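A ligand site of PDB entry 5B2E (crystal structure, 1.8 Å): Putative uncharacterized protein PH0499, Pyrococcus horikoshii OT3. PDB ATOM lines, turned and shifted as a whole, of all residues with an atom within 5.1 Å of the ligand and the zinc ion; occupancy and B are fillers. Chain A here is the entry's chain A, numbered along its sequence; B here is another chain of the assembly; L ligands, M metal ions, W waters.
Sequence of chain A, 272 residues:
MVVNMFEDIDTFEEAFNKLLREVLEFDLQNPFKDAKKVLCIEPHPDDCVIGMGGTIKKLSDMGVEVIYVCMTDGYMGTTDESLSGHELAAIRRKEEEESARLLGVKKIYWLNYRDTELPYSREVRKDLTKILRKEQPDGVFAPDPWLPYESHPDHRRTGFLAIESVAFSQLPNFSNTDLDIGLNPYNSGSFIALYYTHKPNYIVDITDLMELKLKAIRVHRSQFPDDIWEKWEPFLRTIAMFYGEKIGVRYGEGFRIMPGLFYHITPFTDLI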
ATOM      1  N   PRO A  43      -1.062 -10.416  11.075  1.00  0.00           N
ATOM      2  CA  PRO A  43      -0.315 -10.875   9.912  1.00  0.00           C
ATOM      3  C   PRO A  43      -0.055 -12.385  10.006  1.00  0.00           C
ATOM      4  O   PRO A  43      -0.198 -13.074   8.987  1.00  0.00           O
ATOM      5  CB  PRO A  43       1.036 -10.159  10.072  1.00  0.00           C
ATOM      6  CG  PRO A  43       0.605  -8.695  10.887  1.00  0.00           C
ATOM      7  CD  PRO A  43      -0.395  -9.375  11.896  1.00  0.00           C
ATOM      8  N   HIS A  44       0.440 -12.796  11.181  1.00  0.00           N
ATOM      9  CA  HIS A  44       0.764 -14.207  11.447  1.00  0.00           C
ATOM     10  C   HIS A  44       0.045 -14.750  12.622  1.00  0.00           C
ATOM     11  O   HIS A  44      -0.383 -13.994  13.514  1.00  0.00           O
ATOM     12  CB  HIS A  44       2.243 -14.261  11.766  1.00  0.00           C
ATOM     13  CG  HIS A  44       3.085 -13.629  10.738  1.00  0.00           C
ATOM     14  ND1 HIS A  44       3.790 -12.455  10.982  1.00  0.00           N
ATOM     15  CD2 HIS A  44       3.342 -13.975   9.467  1.00  0.00           C
ATOM     16  CE1 HIS A  44       4.414 -12.105   9.840  1.00  0.00           C
ATOM     17  NE2 HIS A  44       4.163 -13.014   8.933  1.00  0.00           N
ATOM     18  N   PRO A  45      -0.025 -16.111  12.708  1.00  0.00           N
ATOM     19  CA  PRO A  45      -0.559 -16.767  13.859  1.00  0.00           C
ATOM     20  C   PRO A  45       0.388 -16.392  15.047  1.00  0.00           C
ATOM     21  O   PRO A  45       1.634 -16.585  14.942  1.00  0.00           O
ATOM     22  CB  PRO A  45      -0.385 -18.290  13.534  1.00  0.00           C
ATOM     23  CG  PRO A  45      -0.100 -18.411  12.096  1.00  0.00           C
ATOM     24  CD  PRO A  45       0.465 -17.029  11.657  1.00  0.00           C
ATOM     25  N   ASP A  46      -0.198 -15.757  16.085  1.00  0.00           N
ATOM     26  CA  ASP A  46       0.448 -15.279  17.352  1.00  0.00           C
ATOM     27  C   ASP A  46       0.456 -13.736  17.455  1.00  0.00           C
ATOM     28  O   ASP A  46       0.732 -13.209  18.530  1.00  0.00           O
ATOM     29  CB  ASP A  46       1.853 -15.830  17.732  1.00  0.00           C
ATOM     30  CG  ASP A  46       2.971 -15.335  16.814  1.00  0.00           C
ATOM     31  OD1 ASP A  46       2.769 -14.290  16.096  1.00  0.00           O
ATOM     32  OD2 ASP A  46       4.126 -15.948  16.794  1.00  0.00           O
ATOM     33  N   ASP A  47       0.207 -13.040  16.369  1.00  0.00           N
ATOM     34  CA  ASP A  47       0.327 -11.572  16.471  1.00  0.00           C
ATOM     35  C   ASP A  47      -0.796 -10.912  17.275  1.00  0.00           C
ATOM     36  O   ASP A  47      -0.558  -9.914  17.953  1.00  0.00           O
ATOM     37  CB  ASP A  47       0.454 -10.886  15.116  1.00  0.00           C
ATOM     38  CG  ASP A  47       1.882 -10.940  14.536  1.00  0.00           C
ATOM     39  OD1 ASP A  47       2.819 -10.503  15.276  1.00  0.00           O
ATOM     40  OD2 ASP A  47       1.943 -11.406  13.360  1.00  0.00           O
ATOM     41  N   ILE A  50       0.368 -11.477  20.881  1.00  0.00           N
ATOM     42  CA  ILE A  50       1.527 -10.736  21.268  1.00  0.00           C
ATOM     43  C   ILE A  50       1.238  -9.244  21.338  1.00  0.00           C
ATOM     44  O   ILE A  50       1.664  -8.593  22.282  1.00  0.00           O
ATOM     45  CB  ILE A  50       2.684 -10.986  20.307  1.00  0.00           C
ATOM     46  CG1 ILE A  50       3.177 -12.440  20.540  1.00  0.00           C
ATOM     47  CG2 ILE A  50       3.828  -9.927  20.491  1.00  0.00           C
ATOM     48  CD1 ILE A  50       4.009 -12.948  19.327  1.00  0.00           C
ATOM     49  N   GLY A  74       1.838 -18.699   8.518  1.00  0.00           N
ATOM     50  CA  GLY A  74       3.058 -18.838   9.311  1.00  0.00           C
ATOM     51  C   GLY A  74       3.953 -19.997   8.831  1.00  0.00           C
ATOM     52  O   GLY A  74       4.820 -20.457   9.557  1.00  0.00           O
ATOM     53  N   MET A  76       6.655 -20.077   7.127  1.00  0.00           N
ATOM     54  CA  MET A  76       8.119 -19.988   7.137  1.00  0.00           C
ATOM     55  C   MET A  76       8.766 -20.002   8.509  1.00  0.00           C
ATOM     56  O   MET A  76       9.982 -20.119   8.591  1.00  0.00           O
ATOM     57  CB  MET A  76       8.599 -18.655   6.389  1.00  0.00           C
ATOM     58  CG  MET A  76       8.205 -18.563   4.917  1.00  0.00           C
ATOM     59  SD  MET A  76       9.141 -19.837   3.928  1.00  0.00           S
ATOM     60  CE  MET A  76       8.379 -19.496   2.317  1.00  0.00           C
ATOM     61  N   GLY A  77       7.987 -19.835   9.599  1.00  0.00           N
ATOM     62  CA  GLY A  77       8.553 -19.515  10.929  1.00  0.00           C
ATOM     63  C   GLY A  77       9.198 -20.718  11.685  1.00  0.00           C
ATOM     64  O   GLY A  77       8.799 -21.026  12.772  1.00  0.00           O
ATOM     65  N   ARG A  92       0.809 -24.626  13.493  1.00  0.00           N
ATOM     66  CA  ARG A  92       0.502 -23.257  14.039  1.00  0.00           C
ATOM     67  C   ARG A  92      -1.011 -22.981  14.055  1.00  0.00           C
ATOM     68  O   ARG A  92      -1.469 -22.239  14.885  1.00  0.00           O
ATOM     69  CB  ARG A  92       1.249 -22.194  13.256  1.00  0.00           C
ATOM     70  CG  ARG A  92       2.832 -22.408  13.340  1.00  0.00           C
ATOM     71  CD  ARG A  92       3.529 -21.228  12.642  1.00  0.00           C
ATOM     72  NE  ARG A  92       3.363 -19.907  13.337  1.00  0.00           N
ATOM     73  CZ  ARG A  92       4.070 -18.846  13.022  1.00  0.00           C
ATOM     74  NH1 ARG A  92       4.966 -18.923  12.049  1.00  0.00           N
ATOM     75  NH2 ARG A  92       3.911 -17.681  13.695  1.00  0.00           N
ATOM     76  N   ASP A 115       2.958 -17.037   4.434  1.00  0.00           N
ATOM     77  CA  ASP A 115       3.948 -16.350   5.215  1.00  0.00           C
ATOM     78  C   ASP A 115       5.155 -15.879   4.363  1.00  0.00           C
ATOM     79  O   ASP A 115       5.781 -16.677   3.639  1.00  0.00           O
ATOM     80  CB  ASP A 115       4.399 -17.326   6.298  1.00  0.00           C
ATOM     81  CG  ASP A 115       5.329 -16.703   7.334  1.00  0.00           C
ATOM     82  OD1 ASP A 115       5.495 -15.452   7.423  1.00  0.00           O
ATOM     83  OD2 ASP A 115       5.903 -17.505   8.117  1.00  0.00           O
ATOM     84  N   THR A 116       5.467 -14.600   4.514  1.00  0.00           N
ATOM     85  CA  THR A 116       6.456 -13.821   3.733  1.00  0.00           C
ATOM     86  C   THR A 116       6.000 -13.417   2.350  1.00  0.00           C
ATOM     87  O   THR A 116       6.770 -12.756   1.607  1.00  0.00           O
ATOM     88  CB  THR A 116       7.867 -14.547   3.601  1.00  0.00           C
ATOM     89  OG1 THR A 116       7.729 -15.609   2.668  1.00  0.00           O
ATOM     90  CG2 THR A 116       8.412 -15.027   5.018  1.00  0.00           C
ATOM     91  N   HIS A 152       9.205  -6.360   8.547  1.00  0.00           N
ATOM     92  CA  HIS A 152       8.444  -7.436   8.024  1.00  0.00           C
ATOM     93  C   HIS A 152       7.352  -6.950   7.068  1.00  0.00           C
ATOM     94  O   HIS A 152       6.367  -6.282   7.571  1.00  0.00           O
ATOM     95  CB  HIS A 152       7.774  -8.260   9.165  1.00  0.00           C
ATOM     96  CG  HIS A 152       7.517  -9.690   8.767  1.00  0.00           C
ATOM     97  ND1 HIS A 152       6.833 -10.059   7.614  1.00  0.00           N
ATOM     98  CD2 HIS A 152       7.966 -10.859   9.323  1.00  0.00           C
ATOM     99  CE1 HIS A 152       6.857 -11.387   7.491  1.00  0.00           C
ATOM    100  NE2 HIS A 152       7.545 -11.890   8.500  1.00  0.00           N
ATOM    101  N   ASP A 154       4.866  -8.519   5.761  1.00  0.00           N
ATOM    102  CA  ASP A 154       3.484  -8.947   6.042  1.00  0.00           C
ATOM    103  C   ASP A 154       2.848  -7.986   7.092  1.00  0.00           C
ATOM    104  O   ASP A 154       1.579  -7.880   7.171  1.00  0.00           O
ATOM    105  CB  ASP A 154       3.487 -10.374   6.614  1.00  0.00           C
ATOM    106  CG  ASP A 154       3.972 -11.443   5.602  1.00  0.00           C
ATOM    107  OD1 ASP A 154       4.311 -12.619   6.086  1.00  0.00           O
ATOM    108  OD2 ASP A 154       3.908 -11.222   4.354  1.00  0.00           O
ATOM    109  N   HIS A 155       3.676  -7.376   7.987  1.00  0.00           N
ATOM    110  CA  HIS A 155       3.151  -6.441   8.993  1.00  0.00           C
ATOM    111  C   HIS A 155       2.694  -5.152   8.355  1.00  0.00           C
ATOM    112  O   HIS A 155       1.570  -4.706   8.603  1.00  0.00           O
ATOM    113  CB  HIS A 155       4.139  -6.247  10.172  1.00  0.00           C
ATOM    114  CG  HIS A 155       4.134  -7.395  11.132  1.00  0.00           C
ATOM    115  ND1 HIS A 155       3.997  -7.242  12.484  1.00  0.00           N
ATOM    116  CD2 HIS A 155       4.098  -8.744  10.895  1.00  0.00           C
ATOM    117  CE1 HIS A 155       3.934  -8.429  13.075  1.00  0.00           C
ATOM    118  NE2 HIS A 155       3.971  -9.349  12.119  1.00  0.00           N
ATOM    119  N   TYR A 196       0.832  -2.526  17.985  1.00  0.00           N
ATOM    120  CA  TYR A 196       2.226  -2.500  17.547  1.00  0.00           C
ATOM    121  C   TYR A 196       2.541  -1.093  17.048  1.00  0.00           C
ATOM    122  O   TYR A 196       2.985  -0.883  15.897  1.00  0.00           O
ATOM    123  CB  TYR A 196       2.474  -3.453  16.424  1.00  0.00           C
ATOM    124  CG  TYR A 196       2.482  -4.960  16.789  1.00  0.00           C
ATOM    125  CD1 TYR A 196       2.886  -5.385  18.022  1.00  0.00           C
ATOM    126  CD2 TYR A 196       2.140  -5.920  15.768  1.00  0.00           C
ATOM    127  CE1 TYR A 196       3.027  -6.758  18.272  1.00  0.00           C
ATOM    128  CE2 TYR A 196       2.233  -7.314  16.034  1.00  0.00           C
ATOM    129  CZ  TYR A 196       2.699  -7.707  17.264  1.00  0.00           C
ATOM    130  OH  TYR A 196       2.813  -9.090  17.439  1.00  0.00           O
ATOM    131  N   GLN A 223       7.090 -21.412  17.877  1.00  0.00           N
ATOM    132  CA  GLN A 223       7.690 -20.084  17.818  1.00  0.00           C
ATOM    133  C   GLN A 223       8.623 -19.760  18.980  1.00  0.00           C
ATOM    134  O   GLN A 223       9.573 -18.947  18.838  1.00  0.00           O
ATOM    135  CB  GLN A 223       6.580 -19.003  17.717  1.00  0.00           C
ATOM    136  CG  GLN A 223       5.685 -19.131  16.447  1.00  0.00           C
ATOM    137  CD  GLN A 223       6.528 -19.312  15.173  1.00  0.00           C
ATOM    138  OE1 GLN A 223       7.191 -18.346  14.699  1.00  0.00           O
ATOM    139  NE2 GLN A 223       6.546 -20.583  14.646  1.00  0.00           N
ATOM    140  N   PHE A 224       8.299 -20.345  20.142  1.00  0.00           N
ATOM    141  CA  PHE A 224       8.908 -19.925  21.384  1.00  0.00           C
ATOM    142  C   PHE A 224       9.534 -21.095  22.164  1.00  0.00           C
ATOM    143  O   PHE A 224       9.101 -21.413  23.279  1.00  0.00           O
ATOM    144  CB  PHE A 224       7.964 -19.025  22.252  1.00  0.00           C
ATOM    145  CG  PHE A 224       7.540 -17.802  21.536  1.00  0.00           C
ATOM    146  CD1 PHE A 224       8.474 -16.795  21.322  1.00  0.00           C
ATOM    147  CD2 PHE A 224       6.269 -17.684  20.963  1.00  0.00           C
ATOM    148  CE1 PHE A 224       8.140 -15.616  20.621  1.00  0.00           C
ATOM    149  CE2 PHE A 224       5.928 -16.543  20.217  1.00  0.00           C
ATOM    150  CZ  PHE A 224       6.867 -15.509  20.028  1.00  0.00           C
ATOM    151  N   TRP A 232      12.852 -13.393  24.189  1.00  0.00           N
ATOM    152  CA  TRP A 232      11.510 -12.838  23.881  1.00  0.00           C
ATOM    153  C   TRP A 232      10.729 -12.409  25.112  1.00  0.00           C
ATOM    154  O   TRP A 232       9.994 -11.374  25.077  1.00  0.00           O
ATOM    155  CB  TRP A 232      10.714 -13.775  22.970  1.00  0.00           C
ATOM    156  CG  TRP A 232      11.011 -13.425  21.527  1.00  0.00           C
ATOM    157  CD1 TRP A 232      12.163 -13.758  20.824  1.00  0.00           C
ATOM    158  CD2 TRP A 232      10.201 -12.690  20.654  1.00  0.00           C
ATOM    159  NE1 TRP A 232      12.082 -13.244  19.559  1.00  0.00           N
ATOM    160  CE2 TRP A 232      10.889 -12.570  19.436  1.00  0.00           C
ATOM    161  CE3 TRP A 232       8.934 -12.065  20.789  1.00  0.00           C
ATOM    162  CZ2 TRP A 232      10.340 -11.913  18.305  1.00  0.00           C
ATOM    163  CZ3 TRP A 232       8.406 -11.404  19.670  1.00  0.00           C
ATOM    164  CH2 TRP A 232       9.106 -11.317  18.466  1.00  0.00           C
ATOM    165  N   PHE B 168      15.074 -13.844   6.159  1.00  0.00           N
ATOM    166  CA  PHE B 168      14.365 -15.022   5.625  1.00  0.00           C
ATOM    167  C   PHE B 168      15.380 -16.074   5.177  1.00  0.00           C
ATOM    168  O   PHE B 168      15.085 -17.255   5.176  1.00  0.00           O
ATOM    169  CB  PHE B 168      13.427 -14.689   4.490  1.00  0.00           C
ATOM    170  CG  PHE B 168      12.322 -13.743   4.903  1.00  0.00           C
ATOM    171  CD1 PHE B 168      11.922 -13.695   6.230  1.00  0.00           C
ATOM    172  CD2 PHE B 168      11.726 -12.903   3.963  1.00  0.00           C
ATOM    173  CE1 PHE B 168      10.888 -12.773   6.684  1.00  0.00           C
ATOM    174  CE2 PHE B 168      10.675 -11.975   4.378  1.00  0.00           C
ATOM    175  CZ  PHE B 168      10.288 -11.914   5.697  1.00  0.00           C
ATOM    176  N   LEU B 171      15.866 -19.167   7.185  1.00  0.00           N
ATOM    177  CA  LEU B 171      14.739 -20.084   7.286  1.00  0.00           C
ATOM    178  C   LEU B 171      14.786 -21.184   6.232  1.00  0.00           C
ATOM    179  O   LEU B 171      14.733 -20.936   5.040  1.00  0.00           O
ATOM    180  CB  LEU B 171      13.407 -19.295   7.187  1.00  0.00           C
ATOM    181  CG  LEU B 171      13.369 -18.120   8.184  1.00  0.00           C
ATOM    182  CD1 LEU B 171      11.950 -17.387   7.947  1.00  0.00           C
ATOM    183  CD2 LEU B 171      13.618 -18.515   9.659  1.00  0.00           C
ATOM    184  N   HIS B 264      11.555  -5.363  14.333  1.00  0.00           N
ATOM    185  CA  HIS B 264      10.190  -5.974  14.267  1.00  0.00           C
ATOM    186  C   HIS B 264       9.449  -5.641  15.548  1.00  0.00           C
ATOM    187  O   HIS B 264       9.969  -5.810  16.666  1.00  0.00           O
ATOM    188  CB  HIS B 264      10.286  -7.542  14.157  1.00  0.00           C
ATOM    189  CG  HIS B 264       8.994  -8.206  13.722  1.00  0.00           C
ATOM    190  ND1 HIS B 264       8.218  -7.741  12.695  1.00  0.00           N
ATOM    191  CD2 HIS B 264       8.381  -9.343  14.169  1.00  0.00           C
ATOM    192  CE1 HIS B 264       7.179  -8.520  12.509  1.00  0.00           C
ATOM    193  NE2 HIS B 264       7.244  -9.495  13.419  1.00  0.00           N
ATOM    194  N   ILE B 265       8.211  -5.146  15.341  1.00  0.00           N
ATOM    195  CA  ILE B 265       7.233  -4.833  16.420  1.00  0.00           C
ATOM    196  C   ILE B 265       7.747  -3.926  17.556  1.00  0.00           C
ATOM    197  O   ILE B 265       7.150  -3.860  18.610  1.00  0.00           O
ATOM    198  CB  ILE B 265       6.489  -6.098  16.968  1.00  0.00           C
ATOM    199  CG1 ILE B 265       7.398  -6.997  17.870  1.00  0.00           C
ATOM    200  CG2 ILE B 265       5.848  -6.804  15.753  1.00  0.00           C
ATOM    201  CD1 ILE B 265       6.558  -8.157  18.628  1.00  0.00           C
HETATM  202  C1  LIG L   1       7.076 -13.963  12.577  1.00  0.00           C
HETATM  203  C2  LIG L   1       6.594 -15.365  12.297  1.00  0.00           C
HETATM  204  C3  LIG L   1       6.792 -15.700  10.825  1.00  0.00           C
HETATM  205  C4  LIG L   1       8.259 -15.353  10.447  1.00  0.00           C
HETATM  206  C5  LIG L   1       8.575 -15.604   8.969  1.00  0.00           C
HETATM  207  C6  LIG L   1       5.793 -12.297  16.249  1.00  0.00           C
HETATM  208  O1  LIG L   1       8.779 -12.436  12.418  1.00  0.00           O
HETATM  209  C7  LIG L   1       8.564 -13.829  12.251  1.00  0.00           C
HETATM  210  O2  LIG L   1       5.168 -15.460  12.653  1.00  0.00           O
HETATM  211  O3  LIG L   1       4.369 -13.573  14.445  1.00  0.00           O
HETATM  212  P1  LIG L   1       5.596 -12.704  14.502  1.00  0.00           P
HETATM  213  O4  LIG L   1       5.382 -11.454  13.595  1.00  0.00           O
HETATM  214  N1  LIG L   1       7.019 -13.575  13.960  1.00  0.00           N
HETATM  215  O5  LIG L   1       6.482 -17.082  10.564  1.00  0.00           O
HETATM  216  O6  LIG L   1       8.684 -13.990  10.863  1.00  0.00           O
HETATM  217  O7  LIG L   1       7.899 -14.609   8.198  1.00  0.00           O
HETATM  218 ZN    ZN M   1       3.787 -11.261  12.633  1.00  0.00          ZN
HETATM  219  O   HOH W   1       9.964 -12.100  14.688  1.00  0.00           O
HETATM  220  O   HOH W   2       6.636 -15.914  15.937  1.00  0.00           O
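A ring nitrogen (NE2) of His 152 lies within hydrogen-bond range of an oxygen (O7) of the ligand.
An oxygen (O5) of the ligand lies within hydrogen-bond range of the side-chain carboxylate (OD2) of Asp 115, at 2.5 Å.
An oxygen (O3) of the ligand lies close to the side-chain carboxylate (OD1) of Asp 46.
The backbone NH of Gly 77 lies close to an oxygen (O5) of the ligand (3.3 Å).
An oxygen (O1) of the ligand sits at hydrogen-bond distance from a ring nitrogen (NE2) of His 264 of chain B (3.5 Å).
NH2 of Arg 92 sits at hydrogen-bond distance from O2 of the ligand (2.8 Å).
NH1 of Arg 92 lies close to NE2 of Gln 223, at 3.5 Å.
The side-chain carboxylate (OD2) of Asp 46 lies within salt-bridge range of the guanidinium group (NH2) of Arg 92 (3.6 Å).
The side-chain carboxylate (OD2) of Asp 115 sits at hydrogen-bond distance from the backbone NH (N) of Gly 77 (3.5 Å).
N of Asp 154 lies within hydrogen-bond range of ND1 of His 152.
The side-chain carboxylate of Asp 47 sits at hydrogen-bond distance from the side-chain hydroxyl of Tyr 196, at 2.6 Å.
The backbone NH (N) of Met 76 is in hydrogen-bond range of the side-chain carboxylate (OD2) of Asp 115.
The backbone carbonyl oxygen of Gly 77 lies within hydrogen-bond range of the side-chain amide nitrogen of Gln 223.
The guanidinium group (NH1) of Arg 92 sits at hydrogen-bond distance from the backbone carbonyl oxygen (O) of Gly 74, 2.9 Å away.
Residues that only touch the ligand: Ile 50 (3.6 Å), Gly 74 (3.9 Å), Met 76 (3.996 Å), Thr 116 (3.2 Å), Gln 223 (3.9 Å), Phe 168 of chain B (3.8 Å) and Leu 171 of chain B (3.95 Å).
Hydrophobic or aromatic side chains that line the ligand: His 44, Ile 50, Met 76, His 152, His 155, Phe 168 of chain B, Leu 171 of chain B and His 264 of chain B.
The nearest printed residue that does not touch the ligand is Pro 45 (4.1 Å).
Residues that only touch the zinc ion: Pro 43 and His 264 of chain B.
Within 4 Å of the zinc ion: Pro 43, His 44, Asp 47, His 155 and His 264 of chain B.
The zinc ion is bound by O4 of the ligand (1.9 Å), OD2 of Asp 47 (2.0 Å), NE2 of His 155 (2.0 Å) and ND1 of His 44 (2.0 Å).
Water W2 lies within hydrogen-bond range of the side-chain carboxylate of Asp 46, the side-chain amide oxygen of Gln 223 and a nitrogen (N1) of the ligand.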
